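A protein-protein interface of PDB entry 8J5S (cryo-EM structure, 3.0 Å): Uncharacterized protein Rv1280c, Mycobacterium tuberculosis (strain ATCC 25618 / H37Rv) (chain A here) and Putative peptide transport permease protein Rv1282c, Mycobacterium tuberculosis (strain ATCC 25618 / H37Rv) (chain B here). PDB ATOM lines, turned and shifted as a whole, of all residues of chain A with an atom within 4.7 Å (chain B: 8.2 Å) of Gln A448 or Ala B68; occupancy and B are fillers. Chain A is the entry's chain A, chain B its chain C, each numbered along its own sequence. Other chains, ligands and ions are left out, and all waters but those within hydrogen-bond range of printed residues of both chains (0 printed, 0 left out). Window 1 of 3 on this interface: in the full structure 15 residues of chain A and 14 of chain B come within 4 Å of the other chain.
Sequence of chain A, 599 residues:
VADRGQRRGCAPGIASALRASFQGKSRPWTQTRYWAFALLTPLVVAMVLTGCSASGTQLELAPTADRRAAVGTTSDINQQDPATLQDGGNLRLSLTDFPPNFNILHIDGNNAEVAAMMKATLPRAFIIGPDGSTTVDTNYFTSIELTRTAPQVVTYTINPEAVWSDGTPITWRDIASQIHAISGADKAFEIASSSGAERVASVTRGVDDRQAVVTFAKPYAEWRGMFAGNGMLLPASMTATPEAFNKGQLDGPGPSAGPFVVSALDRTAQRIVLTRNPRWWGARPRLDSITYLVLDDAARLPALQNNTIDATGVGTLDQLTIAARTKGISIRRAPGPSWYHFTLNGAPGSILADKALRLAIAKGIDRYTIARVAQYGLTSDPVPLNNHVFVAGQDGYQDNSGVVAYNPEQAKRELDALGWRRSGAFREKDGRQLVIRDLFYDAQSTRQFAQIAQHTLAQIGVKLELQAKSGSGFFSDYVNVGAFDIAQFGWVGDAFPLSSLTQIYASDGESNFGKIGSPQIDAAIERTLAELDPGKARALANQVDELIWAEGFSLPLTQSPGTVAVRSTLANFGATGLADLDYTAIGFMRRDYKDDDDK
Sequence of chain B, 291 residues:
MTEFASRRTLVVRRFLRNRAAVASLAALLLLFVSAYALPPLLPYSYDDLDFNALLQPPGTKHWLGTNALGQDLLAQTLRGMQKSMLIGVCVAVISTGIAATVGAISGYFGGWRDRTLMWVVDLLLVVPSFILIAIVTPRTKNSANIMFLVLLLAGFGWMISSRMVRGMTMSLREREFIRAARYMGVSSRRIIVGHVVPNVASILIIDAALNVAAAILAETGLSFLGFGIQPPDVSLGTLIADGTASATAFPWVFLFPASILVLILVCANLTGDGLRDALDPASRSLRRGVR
CG2 of Val A373 touches CD2 of Phe B51 (3.5 Å).
Gln A448 touches Ala B68 (NE2 to CB, 3.6 Å).
Gln A451 touches Leu B69.
Leu B49 touches Ile A452.
Leu B69 touches Ile A452.
Of chain A, only Gln A448 (3.6 Å) comes within 4 Å of Ala B68.
Printed residues of chain B within 4 Å of Val A373: Phe B51 (3.5 Å).
Of the printed residues of chain B, Ile A452 touches Leu B49 (3.9 Å) and Leu B69 (3.6 Å).
Of the printed residues of chain A, Leu B69 touches Gln A451 and Ile A452.
The nearest printed residue of chain B that does not touch Gln A448 is Leu B69 (4.02 Å).
The nearest residue of chain A that does not touch Ala B68 is Val A373 (4.2 Å).
The nearest printed residue of chain A that does not touch Leu B49 is Gln A451 (5.7 Å).
Printed residues of chain A that touch a printed residue of chain B: Val A373, Gln A448, Gln A451 and Ile A452.
Printed residues of chain B that touch a printed residue of chain A: Leu B49, Phe B51, Ala B68 and Leu B69.
Hydrophobic or aromatic side chains of chain B that line the printed part of chain A: Leu B49, Phe B51, Ala B68 and Leu B69.
Among the printed residues, 5 pairs touch across the chains.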
ATOM      1  N   THR A 316      15.079 -23.873  -2.888  1.00  0.00           N
ATOM      2  CA  THR A 316      15.395 -24.932  -1.945  1.00  0.00           C
ATOM      3  C   THR A 316      14.131 -25.701  -1.603  1.00  0.00           C
ATOM      4  O   THR A 316      13.059 -25.449  -2.150  1.00  0.00           O
ATOM      5  CB  THR A 316      16.048 -24.371  -0.677  1.00  0.00           C
ATOM      6  OG1 THR A 316      15.249 -23.307  -0.155  1.00  0.00           O
ATOM      7  CG2 THR A 316      17.432 -23.848  -0.979  1.00  0.00           C
ATOM      8  N   VAL A 373      22.823 -32.511  -2.681  1.00  0.00           N
ATOM      9  CA  VAL A 373      22.400 -31.678  -1.562  1.00  0.00           C
ATOM     10  C   VAL A 373      21.636 -30.458  -2.053  1.00  0.00           C
ATOM     11  O   VAL A 373      20.635 -30.058  -1.453  1.00  0.00           O
ATOM     12  CB  VAL A 373      23.611 -31.276  -0.708  1.00  0.00           C
ATOM     13  CG1 VAL A 373      23.249 -30.136   0.214  1.00  0.00           C
ATOM     14  CG2 VAL A 373      24.105 -32.466   0.079  1.00  0.00           C
ATOM     15  N   GLN A 444      19.791 -18.057   0.577  1.00  0.00           N
ATOM     16  CA  GLN A 444      19.619 -19.313   1.293  1.00  0.00           C
ATOM     17  C   GLN A 444      20.152 -20.494   0.501  1.00  0.00           C
ATOM     18  O   GLN A 444      20.721 -21.422   1.080  1.00  0.00           O
ATOM     19  CB  GLN A 444      18.143 -19.534   1.630  1.00  0.00           C
ATOM     20  CG  GLN A 444      17.877 -20.791   2.444  1.00  0.00           C
ATOM     21  CD  GLN A 444      16.462 -21.304   2.286  1.00  0.00           C
ATOM     22  OE1 GLN A 444      16.244 -22.483   2.013  1.00  0.00           O
ATOM     23  NE2 GLN A 444      15.489 -20.418   2.460  1.00  0.00           N
ATOM     24  N   SER A 445      19.979 -20.472  -0.815  1.00  0.00           N
ATOM     25  CA  SER A 445      20.417 -21.566  -1.666  1.00  0.00           C
ATOM     26  C   SER A 445      21.874 -21.453  -2.075  1.00  0.00           C
ATOM     27  O   SER A 445      22.542 -22.477  -2.232  1.00  0.00           O
ATOM     28  CB  SER A 445      19.547 -21.630  -2.922  1.00  0.00           C
ATOM     29  OG  SER A 445      19.376 -20.342  -3.482  1.00  0.00           O
ATOM     30  N   THR A 446      22.378 -20.234  -2.260  1.00  0.00           N
ATOM     31  CA  THR A 446      23.723 -20.069  -2.791  1.00  0.00           C
ATOM     32  C   THR A 446      24.788 -20.399  -1.762  1.00  0.00           C
ATOM     33  O   THR A 446      25.876 -20.852  -2.130  1.00  0.00           O
ATOM     34  CB  THR A 446      23.928 -18.651  -3.301  1.00  0.00           C
ATOM     35  OG1 THR A 446      24.232 -17.795  -2.201  1.00  0.00           O
ATOM     36  CG2 THR A 446      22.691 -18.158  -3.996  1.00  0.00           C
ATOM     37  N   ARG A 447      24.514 -20.176  -0.483  1.00  0.00           N
ATOM     38  CA  ARG A 447      25.536 -20.463   0.511  1.00  0.00           C
ATOM     39  C   ARG A 447      25.668 -21.943   0.807  1.00  0.00           C
ATOM     40  O   ARG A 447      26.702 -22.353   1.332  1.00  0.00           O
ATOM     41  CB  ARG A 447      25.265 -19.700   1.803  1.00  0.00           C
ATOM     42  CG  ARG A 447      23.901 -19.905   2.386  1.00  0.00           C
ATOM     43  CD  ARG A 447      23.804 -19.288   3.771  1.00  0.00           C
ATOM     44  NE  ARG A 447      24.474 -17.994   3.863  1.00  0.00           N
ATOM     45  CZ  ARG A 447      25.601 -17.780   4.536  1.00  0.00           C
ATOM     46  NH1 ARG A 447      26.197 -18.779   5.168  1.00  0.00           N
ATOM     47  NH2 ARG A 447      26.137 -16.567   4.572  1.00  0.00           N
ATOM     48  N   GLN A 448      24.667 -22.753   0.473  1.00  0.00           N
ATOM     49  CA  GLN A 448      24.801 -24.194   0.656  1.00  0.00           C
ATOM     50  C   GLN A 448      25.906 -24.760  -0.220  1.00  0.00           C
ATOM     51  O   GLN A 448      26.670 -25.628   0.214  1.00  0.00           O
ATOM     52  CB  GLN A 448      23.477 -24.888   0.361  1.00  0.00           C
ATOM     53  CG  GLN A 448      22.657 -25.180   1.599  1.00  0.00           C
ATOM     54  CD  GLN A 448      21.183 -25.261   1.309  1.00  0.00           C
ATOM     55  OE1 GLN A 448      20.776 -25.463   0.169  1.00  0.00           O
ATOM     56  NE2 GLN A 448      20.369 -25.089   2.339  1.00  0.00           N
ATOM     57  N   PHE A 449      26.004 -24.283  -1.460  1.00  0.00           N
ATOM     58  CA  PHE A 449      27.105 -24.679  -2.330  1.00  0.00           C
ATOM     59  C   PHE A 449      28.440 -24.358  -1.684  1.00  0.00           C
ATOM     60  O   PHE A 449      29.360 -25.179  -1.689  1.00  0.00           O
ATOM     61  CB  PHE A 449      27.001 -23.959  -3.670  1.00  0.00           C
ATOM     62  CG  PHE A 449      25.820 -24.353  -4.490  1.00  0.00           C
ATOM     63  CD1 PHE A 449      25.901 -25.397  -5.377  1.00  0.00           C
ATOM     64  CD2 PHE A 449      24.640 -23.656  -4.398  1.00  0.00           C
ATOM     65  CE1 PHE A 449      24.825 -25.748  -6.143  1.00  0.00           C
ATOM     66  CE2 PHE A 449      23.563 -24.005  -5.162  1.00  0.00           C
ATOM     67  CZ  PHE A 449      23.657 -25.049  -6.037  1.00  0.00           C
ATOM     68  N   ALA A 450      28.560 -23.157  -1.126  1.00  0.00           N
ATOM     69  CA  ALA A 450      29.808 -22.738  -0.509  1.00  0.00           C
ATOM     70  C   ALA A 450      30.158 -23.611   0.682  1.00  0.00           C
ATOM     71  O   ALA A 450      31.313 -24.007   0.849  1.00  0.00           O
ATOM     72  CB  ALA A 450      29.707 -21.278  -0.087  1.00  0.00           C
ATOM     73  N   GLN A 451      29.175 -23.924   1.524  1.00  0.00           N
ATOM     74  CA  GLN A 451      29.459 -24.736   2.701  1.00  0.00           C
ATOM     75  C   GLN A 451      29.868 -26.149   2.319  1.00  0.00           C
ATOM     76  O   GLN A 451      30.825 -26.689   2.880  1.00  0.00           O
ATOM     77  CB  GLN A 451      28.256 -24.754   3.631  1.00  0.00           C
ATOM     78  CG  GLN A 451      27.676 -23.391   3.873  1.00  0.00           C
ATOM     79  CD  GLN A 451      27.111 -23.222   5.252  1.00  0.00           C
ATOM     80  OE1 GLN A 451      27.765 -23.530   6.242  1.00  0.00           O
ATOM     81  NE2 GLN A 451      25.883 -22.727   5.332  1.00  0.00           N
ATOM     82  N   ILE A 452      29.173 -26.766   1.363  1.00  0.00           N
ATOM     83  CA  ILE A 452      29.572 -28.107   0.940  1.00  0.00           C
ATOM     84  C   ILE A 452      30.960 -28.077   0.325  1.00  0.00           C
ATOM     85  O   ILE A 452      31.786 -28.960   0.580  1.00  0.00           O
ATOM     86  CB  ILE A 452      28.547 -28.713  -0.032  1.00  0.00           C
ATOM     87  CG1 ILE A 452      27.141 -28.646   0.544  1.00  0.00           C
ATOM     88  CG2 ILE A 452      28.894 -30.149  -0.322  1.00  0.00           C
ATOM     89  CD1 ILE A 452      26.947 -29.490   1.762  1.00  0.00           C
ATOM     90  N   LEU B  49      29.044 -34.748   7.610  1.00  0.00           N
ATOM     91  CA  LEU B  49      27.768 -34.642   6.921  1.00  0.00           C
ATOM     92  C   LEU B  49      27.257 -36.016   6.515  1.00  0.00           C
ATOM     93  O   LEU B  49      28.023 -36.860   6.048  1.00  0.00           O
ATOM     94  CB  LEU B  49      27.896 -33.772   5.674  1.00  0.00           C
ATOM     95  CG  LEU B  49      28.591 -32.423   5.808  1.00  0.00           C
ATOM     96  CD1 LEU B  49      28.570 -31.652   4.508  1.00  0.00           C
ATOM     97  CD2 LEU B  49      27.908 -31.644   6.837  1.00  0.00           C
ATOM     98  N   ASP B  50      25.955 -36.227   6.684  1.00  0.00           N
ATOM     99  CA  ASP B  50      25.278 -37.426   6.207  1.00  0.00           C
ATOM    100  C   ASP B  50      24.437 -37.035   5.002  1.00  0.00           C
ATOM    101  O   ASP B  50      23.448 -36.313   5.139  1.00  0.00           O
ATOM    102  CB  ASP B  50      24.421 -38.047   7.304  1.00  0.00           C
ATOM    103  CG  ASP B  50      24.359 -39.549   7.204  1.00  0.00           C
ATOM    104  OD1 ASP B  50      24.446 -40.226   8.244  1.00  0.00           O
ATOM    105  OD2 ASP B  50      24.233 -40.059   6.079  1.00  0.00           O
ATOM    106  N   PHE B  51      24.831 -37.506   3.825  1.00  0.00           N
ATOM    107  CA  PHE B  51      24.263 -37.021   2.579  1.00  0.00           C
ATOM    108  C   PHE B  51      23.055 -37.811   2.113  1.00  0.00           C
ATOM    109  O   PHE B  51      22.429 -37.418   1.127  1.00  0.00           O
ATOM    110  CB  PHE B  51      25.331 -37.027   1.482  1.00  0.00           C
ATOM    111  CG  PHE B  51      26.440 -36.051   1.719  1.00  0.00           C
ATOM    112  CD1 PHE B  51      27.742 -36.479   1.830  1.00  0.00           C
ATOM    113  CD2 PHE B  51      26.176 -34.704   1.843  1.00  0.00           C
ATOM    114  CE1 PHE B  51      28.755 -35.582   2.052  1.00  0.00           C
ATOM    115  CE2 PHE B  51      27.184 -33.807   2.065  1.00  0.00           C
ATOM    116  CZ  PHE B  51      28.475 -34.245   2.166  1.00  0.00           C
ATOM    117  N   ALA B  53      20.736 -38.557   4.611  1.00  0.00           N
ATOM    118  CA  ALA B  53      19.933 -38.296   5.795  1.00  0.00           C
ATOM    119  C   ALA B  53      19.625 -36.814   5.889  1.00  0.00           C
ATOM    120  O   ALA B  53      19.850 -36.168   6.910  1.00  0.00           O
ATOM    121  CB  ALA B  53      20.639 -38.781   7.053  1.00  0.00           C
ATOM    122  N   LEU B  54      19.128 -36.245   4.798  1.00  0.00           N
ATOM    123  CA  LEU B  54      18.938 -34.808   4.692  1.00  0.00           C
ATOM    124  C   LEU B  54      17.582 -34.396   5.248  1.00  0.00           C
ATOM    125  O   LEU B  54      16.551 -34.944   4.854  1.00  0.00           O
ATOM    126  CB  LEU B  54      19.061 -34.371   3.235  1.00  0.00           C
ATOM    127  CG  LEU B  54      20.464 -34.242   2.663  1.00  0.00           C
ATOM    128  CD1 LEU B  54      20.432 -34.460   1.186  1.00  0.00           C
ATOM    129  CD2 LEU B  54      20.998 -32.883   2.969  1.00  0.00           C
ATOM    130  N   LEU B  55      17.597 -33.428   6.161  1.00  0.00           N
ATOM    131  CA  LEU B  55      16.390 -32.846   6.752  1.00  0.00           C
ATOM    132  C   LEU B  55      15.471 -33.907   7.346  1.00  0.00           C
ATOM    133  O   LEU B  55      14.257 -33.881   7.160  1.00  0.00           O
ATOM    134  CB  LEU B  55      15.661 -31.988   5.734  1.00  0.00           C
ATOM    135  CG  LEU B  55      16.186 -30.558   5.775  1.00  0.00           C
ATOM    136  CD1 LEU B  55      15.444 -29.663   4.833  1.00  0.00           C
ATOM    137  CD2 LEU B  55      16.107 -30.017   7.180  1.00  0.00           C
ATOM    138  N   GLN B  56      16.059 -34.846   8.078  1.00  0.00           N
ATOM    139  CA  GLN B  56      15.321 -35.902   8.742  1.00  0.00           C
ATOM    140  C   GLN B  56      14.748 -35.411  10.066  1.00  0.00           C
ATOM    141  O   GLN B  56      15.328 -34.541  10.714  1.00  0.00           O
ATOM    142  CB  GLN B  56      16.222 -37.096   9.004  1.00  0.00           C
ATOM    143  CG  GLN B  56      16.869 -37.663   7.781  1.00  0.00           C
ATOM    144  CD  GLN B  56      15.918 -38.480   6.955  1.00  0.00           C
ATOM    145  OE1 GLN B  56      15.001 -37.946   6.337  1.00  0.00           O
ATOM    146  NE2 GLN B  56      16.129 -39.788   6.935  1.00  0.00           N
ATOM    147  N   GLY B  65      17.421 -34.784  14.974  1.00  0.00           N
ATOM    148  CA  GLY B  65      17.133 -34.507  13.572  1.00  0.00           C
ATOM    149  C   GLY B  65      18.347 -34.055  12.840  1.00  0.00           C
ATOM    150  O   GLY B  65      19.367 -33.908  13.480  1.00  0.00           O
ATOM    151  N   THR B  66      18.216 -33.859  11.537  1.00  0.00           N
ATOM    152  CA  THR B  66      19.310 -33.383  10.727  1.00  0.00           C
ATOM    153  C   THR B  66      18.998 -31.984  10.234  1.00  0.00           C
ATOM    154  O   THR B  66      18.054 -31.334  10.677  1.00  0.00           O
ATOM    155  CB  THR B  66      19.572 -34.333   9.574  1.00  0.00           C
ATOM    156  OG1 THR B  66      18.349 -34.582   8.891  1.00  0.00           O
ATOM    157  CG2 THR B  66      20.118 -35.622  10.089  1.00  0.00           C
ATOM    158  N   ASN B  67      19.804 -31.516   9.304  1.00  0.00           N
ATOM    159  CA  ASN B  67      19.839 -30.136   8.876  1.00  0.00           C
ATOM    160  C   ASN B  67      19.733 -30.118   7.359  1.00  0.00           C
ATOM    161  O   ASN B  67      19.790 -31.159   6.705  1.00  0.00           O
ATOM    162  CB  ASN B  67      21.129 -29.484   9.399  1.00  0.00           C
ATOM    163  CG  ASN B  67      21.466 -28.204   8.723  1.00  0.00           C
ATOM    164  OD1 ASN B  67      20.594 -27.504   8.223  1.00  0.00           O
ATOM    165  ND2 ASN B  67      22.741 -27.882   8.690  1.00  0.00           N
ATOM    166  N   ALA B  68      19.556 -28.924   6.795  1.00  0.00           N
ATOM    167  CA  ALA B  68      19.504 -28.789   5.345  1.00  0.00           C
ATOM    168  C   ALA B  68      20.736 -29.369   4.677  1.00  0.00           C
ATOM    169  O   ALA B  68      20.661 -29.822   3.535  1.00  0.00           O
ATOM    170  CB  ALA B  68      19.350 -27.322   4.962  1.00  0.00           C
ATOM    171  N   LEU B  69      21.874 -29.359   5.368  1.00  0.00           N
ATOM    172  CA  LEU B  69      23.136 -29.865   4.848  1.00  0.00           C
ATOM    173  C   LEU B  69      23.487 -31.247   5.374  1.00  0.00           C
ATOM    174  O   LEU B  69      24.577 -31.741   5.091  1.00  0.00           O
ATOM    175  CB  LEU B  69      24.262 -28.894   5.178  1.00  0.00           C
ATOM    176  CG  LEU B  69      24.243 -27.551   4.464  1.00  0.00           C
ATOM    177  CD1 LEU B  69      23.525 -26.507   5.289  1.00  0.00           C
ATOM    178  CD2 LEU B  69      25.651 -27.122   4.194  1.00  0.00           C
ATOM    179  N   GLY B  70      22.601 -31.878   6.132  1.00  0.00           N
ATOM    180  CA  GLY B  70      22.839 -33.224   6.602  1.00  0.00           C
ATOM    181  C   GLY B  70      23.603 -33.342   7.896  1.00  0.00           C
ATOM    182  O   GLY B  70      24.104 -34.427   8.203  1.00  0.00           O
ATOM    183  N   GLN B  71      23.711 -32.270   8.668  1.00  0.00           N
ATOM    184  CA  GLN B  71      24.425 -32.296   9.933  1.00  0.00           C
ATOM    185  C   GLN B  71      23.492 -32.695  11.058  1.00  0.00           C
ATOM    186  O   GLN B  71      22.337 -32.271  11.095  1.00  0.00           O
ATOM    187  CB  GLN B  71      25.030 -30.928  10.235  1.00  0.00           C
ATOM    188  CG  GLN B  71      26.118 -30.550   9.295  1.00  0.00           C
ATOM    189  CD  GLN B  71      26.314 -29.072   9.136  1.00  0.00           C
ATOM    190  OE1 GLN B  71      25.425 -28.290   9.435  1.00  0.00           O
ATOM    191  NE2 GLN B  71      27.467 -28.679   8.650  1.00  0.00           N
ATOM    192  N   LEU B  73      21.769 -32.252  14.279  1.00  0.00           N
ATOM    193  CA  LEU B  73      21.492 -31.006  14.967  1.00  0.00           C
ATOM    194  C   LEU B  73      21.747 -31.086  16.463  1.00  0.00           C
ATOM    195  O   LEU B  73      21.585 -30.078  17.149  1.00  0.00           O
ATOM    196  CB  LEU B  73      20.055 -30.578  14.699  1.00  0.00           C
ATOM    197  CG  LEU B  73      19.776 -29.101  14.908  1.00  0.00           C
ATOM    198  CD1 LEU B  73      20.379 -28.270  13.803  1.00  0.00           C
ATOM    199  CD2 LEU B  73      18.320 -28.921  14.953  1.00  0.00           C
ATOM    200  N   ASP B 242      20.904 -19.567  10.823  1.00  0.00           N
ATOM    201  CA  ASP B 242      20.701 -20.536   9.754  1.00  0.00           C
ATOM    202  C   ASP B 242      19.302 -21.123   9.802  1.00  0.00           C
ATOM    203  O   ASP B 242      18.680 -21.342   8.759  1.00  0.00           O
ATOM    204  CB  ASP B 242      21.735 -21.653   9.845  1.00  0.00           C
ATOM    205  CG  ASP B 242      23.153 -21.141   9.797  1.00  0.00           C
ATOM    206  OD1 ASP B 242      24.086 -21.963   9.903  1.00  0.00           O
ATOM    207  OD2 ASP B 242      23.336 -19.914   9.658  1.00  0.00           O
ATOM    208  N   SER B 246      13.654 -22.084   8.111  1.00  0.00           N
ATOM    209  CA  SER B 246      13.008 -23.382   7.985  1.00  0.00           C
ATOM    210  C   SER B 246      12.179 -23.751   9.206  1.00  0.00           C
ATOM    211  O   SER B 246      11.809 -24.920   9.349  1.00  0.00           O
ATOM    212  CB  SER B 246      14.048 -24.467   7.728  1.00  0.00           C
ATOM    213  OG  SER B 246      14.853 -24.140   6.612  1.00  0.00           O
ATOM    214  N   PHE B 250      10.184 -27.452   8.810  1.00  0.00           N
ATOM    215  CA  PHE B 250      10.900 -28.412   9.650  1.00  0.00           C
ATOM    216  C   PHE B 250      11.312 -27.668  10.909  1.00  0.00           C
ATOM    217  O   PHE B 250      12.412 -27.104  10.969  1.00  0.00           O
ATOM    218  CB  PHE B 250      12.115 -28.988   8.935  1.00  0.00           C
ATOM    219  CG  PHE B 250      11.904 -29.207   7.473  1.00  0.00           C
ATOM    220  CD1 PHE B 250      12.545 -28.431   6.542  1.00  0.00           C
ATOM    221  CD2 PHE B 250      11.067 -30.202   7.026  1.00  0.00           C
ATOM    222  CE1 PHE B 250      12.341 -28.642   5.201  1.00  0.00           C
ATOM    223  CE2 PHE B 250      10.872 -30.408   5.685  1.00  0.00           C
ATOM    224  CZ  PHE B 250      11.514 -29.624   4.776  1.00  0.00           C
ATOM    225  N   TRP B 252      12.296 -28.476  13.848  1.00  0.00           N
ATOM    226  CA  TRP B 252      13.340 -28.954  14.737  1.00  0.00           C
ATOM    227  C   TRP B 252      14.655 -28.222  14.532  1.00  0.00           C
ATOM    228  O   TRP B 252      15.484 -28.218  15.442  1.00  0.00           O
ATOM    229  CB  TRP B 252      13.536 -30.463  14.575  1.00  0.00           C
ATOM    230  CG  TRP B 252      13.936 -30.926  13.210  1.00  0.00           C
ATOM    231  CD1 TRP B 252      15.170 -30.861  12.654  1.00  0.00           C
ATOM    232  CD2 TRP B 252      13.096 -31.556  12.238  1.00  0.00           C
ATOM    233  NE1 TRP B 252      15.154 -31.395  11.395  1.00  0.00           N
ATOM    234  CE2 TRP B 252      13.890 -31.832  11.118  1.00  0.00           C
ATOM    235  CE3 TRP B 252      11.744 -31.906  12.206  1.00  0.00           C
ATOM    236  CZ2 TRP B 252      13.380 -32.430   9.978  1.00  0.00           C
ATOM    237  CZ3 TRP B 252      11.243 -32.507  11.079  1.00  0.00           C
ATOM    238  CH2 TRP B 252      12.056 -32.765   9.980  1.00  0.00           C
ATOM    239  N   VAL B 253      14.851 -27.570  13.379  1.00  0.00           N
ATOM    240  CA  VAL B 253      16.117 -26.900  13.086  1.00  0.00           C
ATOM    241  C   VAL B 253      16.199 -25.493  13.650  1.00  0.00           C
ATOM    242  O   VAL B 253      17.292 -24.911  13.667  1.00  0.00           O
ATOM    243  CB  VAL B 253      16.392 -26.818  11.572  1.00  0.00           C
ATOM    244  CG1 VAL B 253      16.341 -28.188  10.946  1.00  0.00           C
ATOM    245  CG2 VAL B 253      15.414 -25.894  10.912  1.00  0.00           C
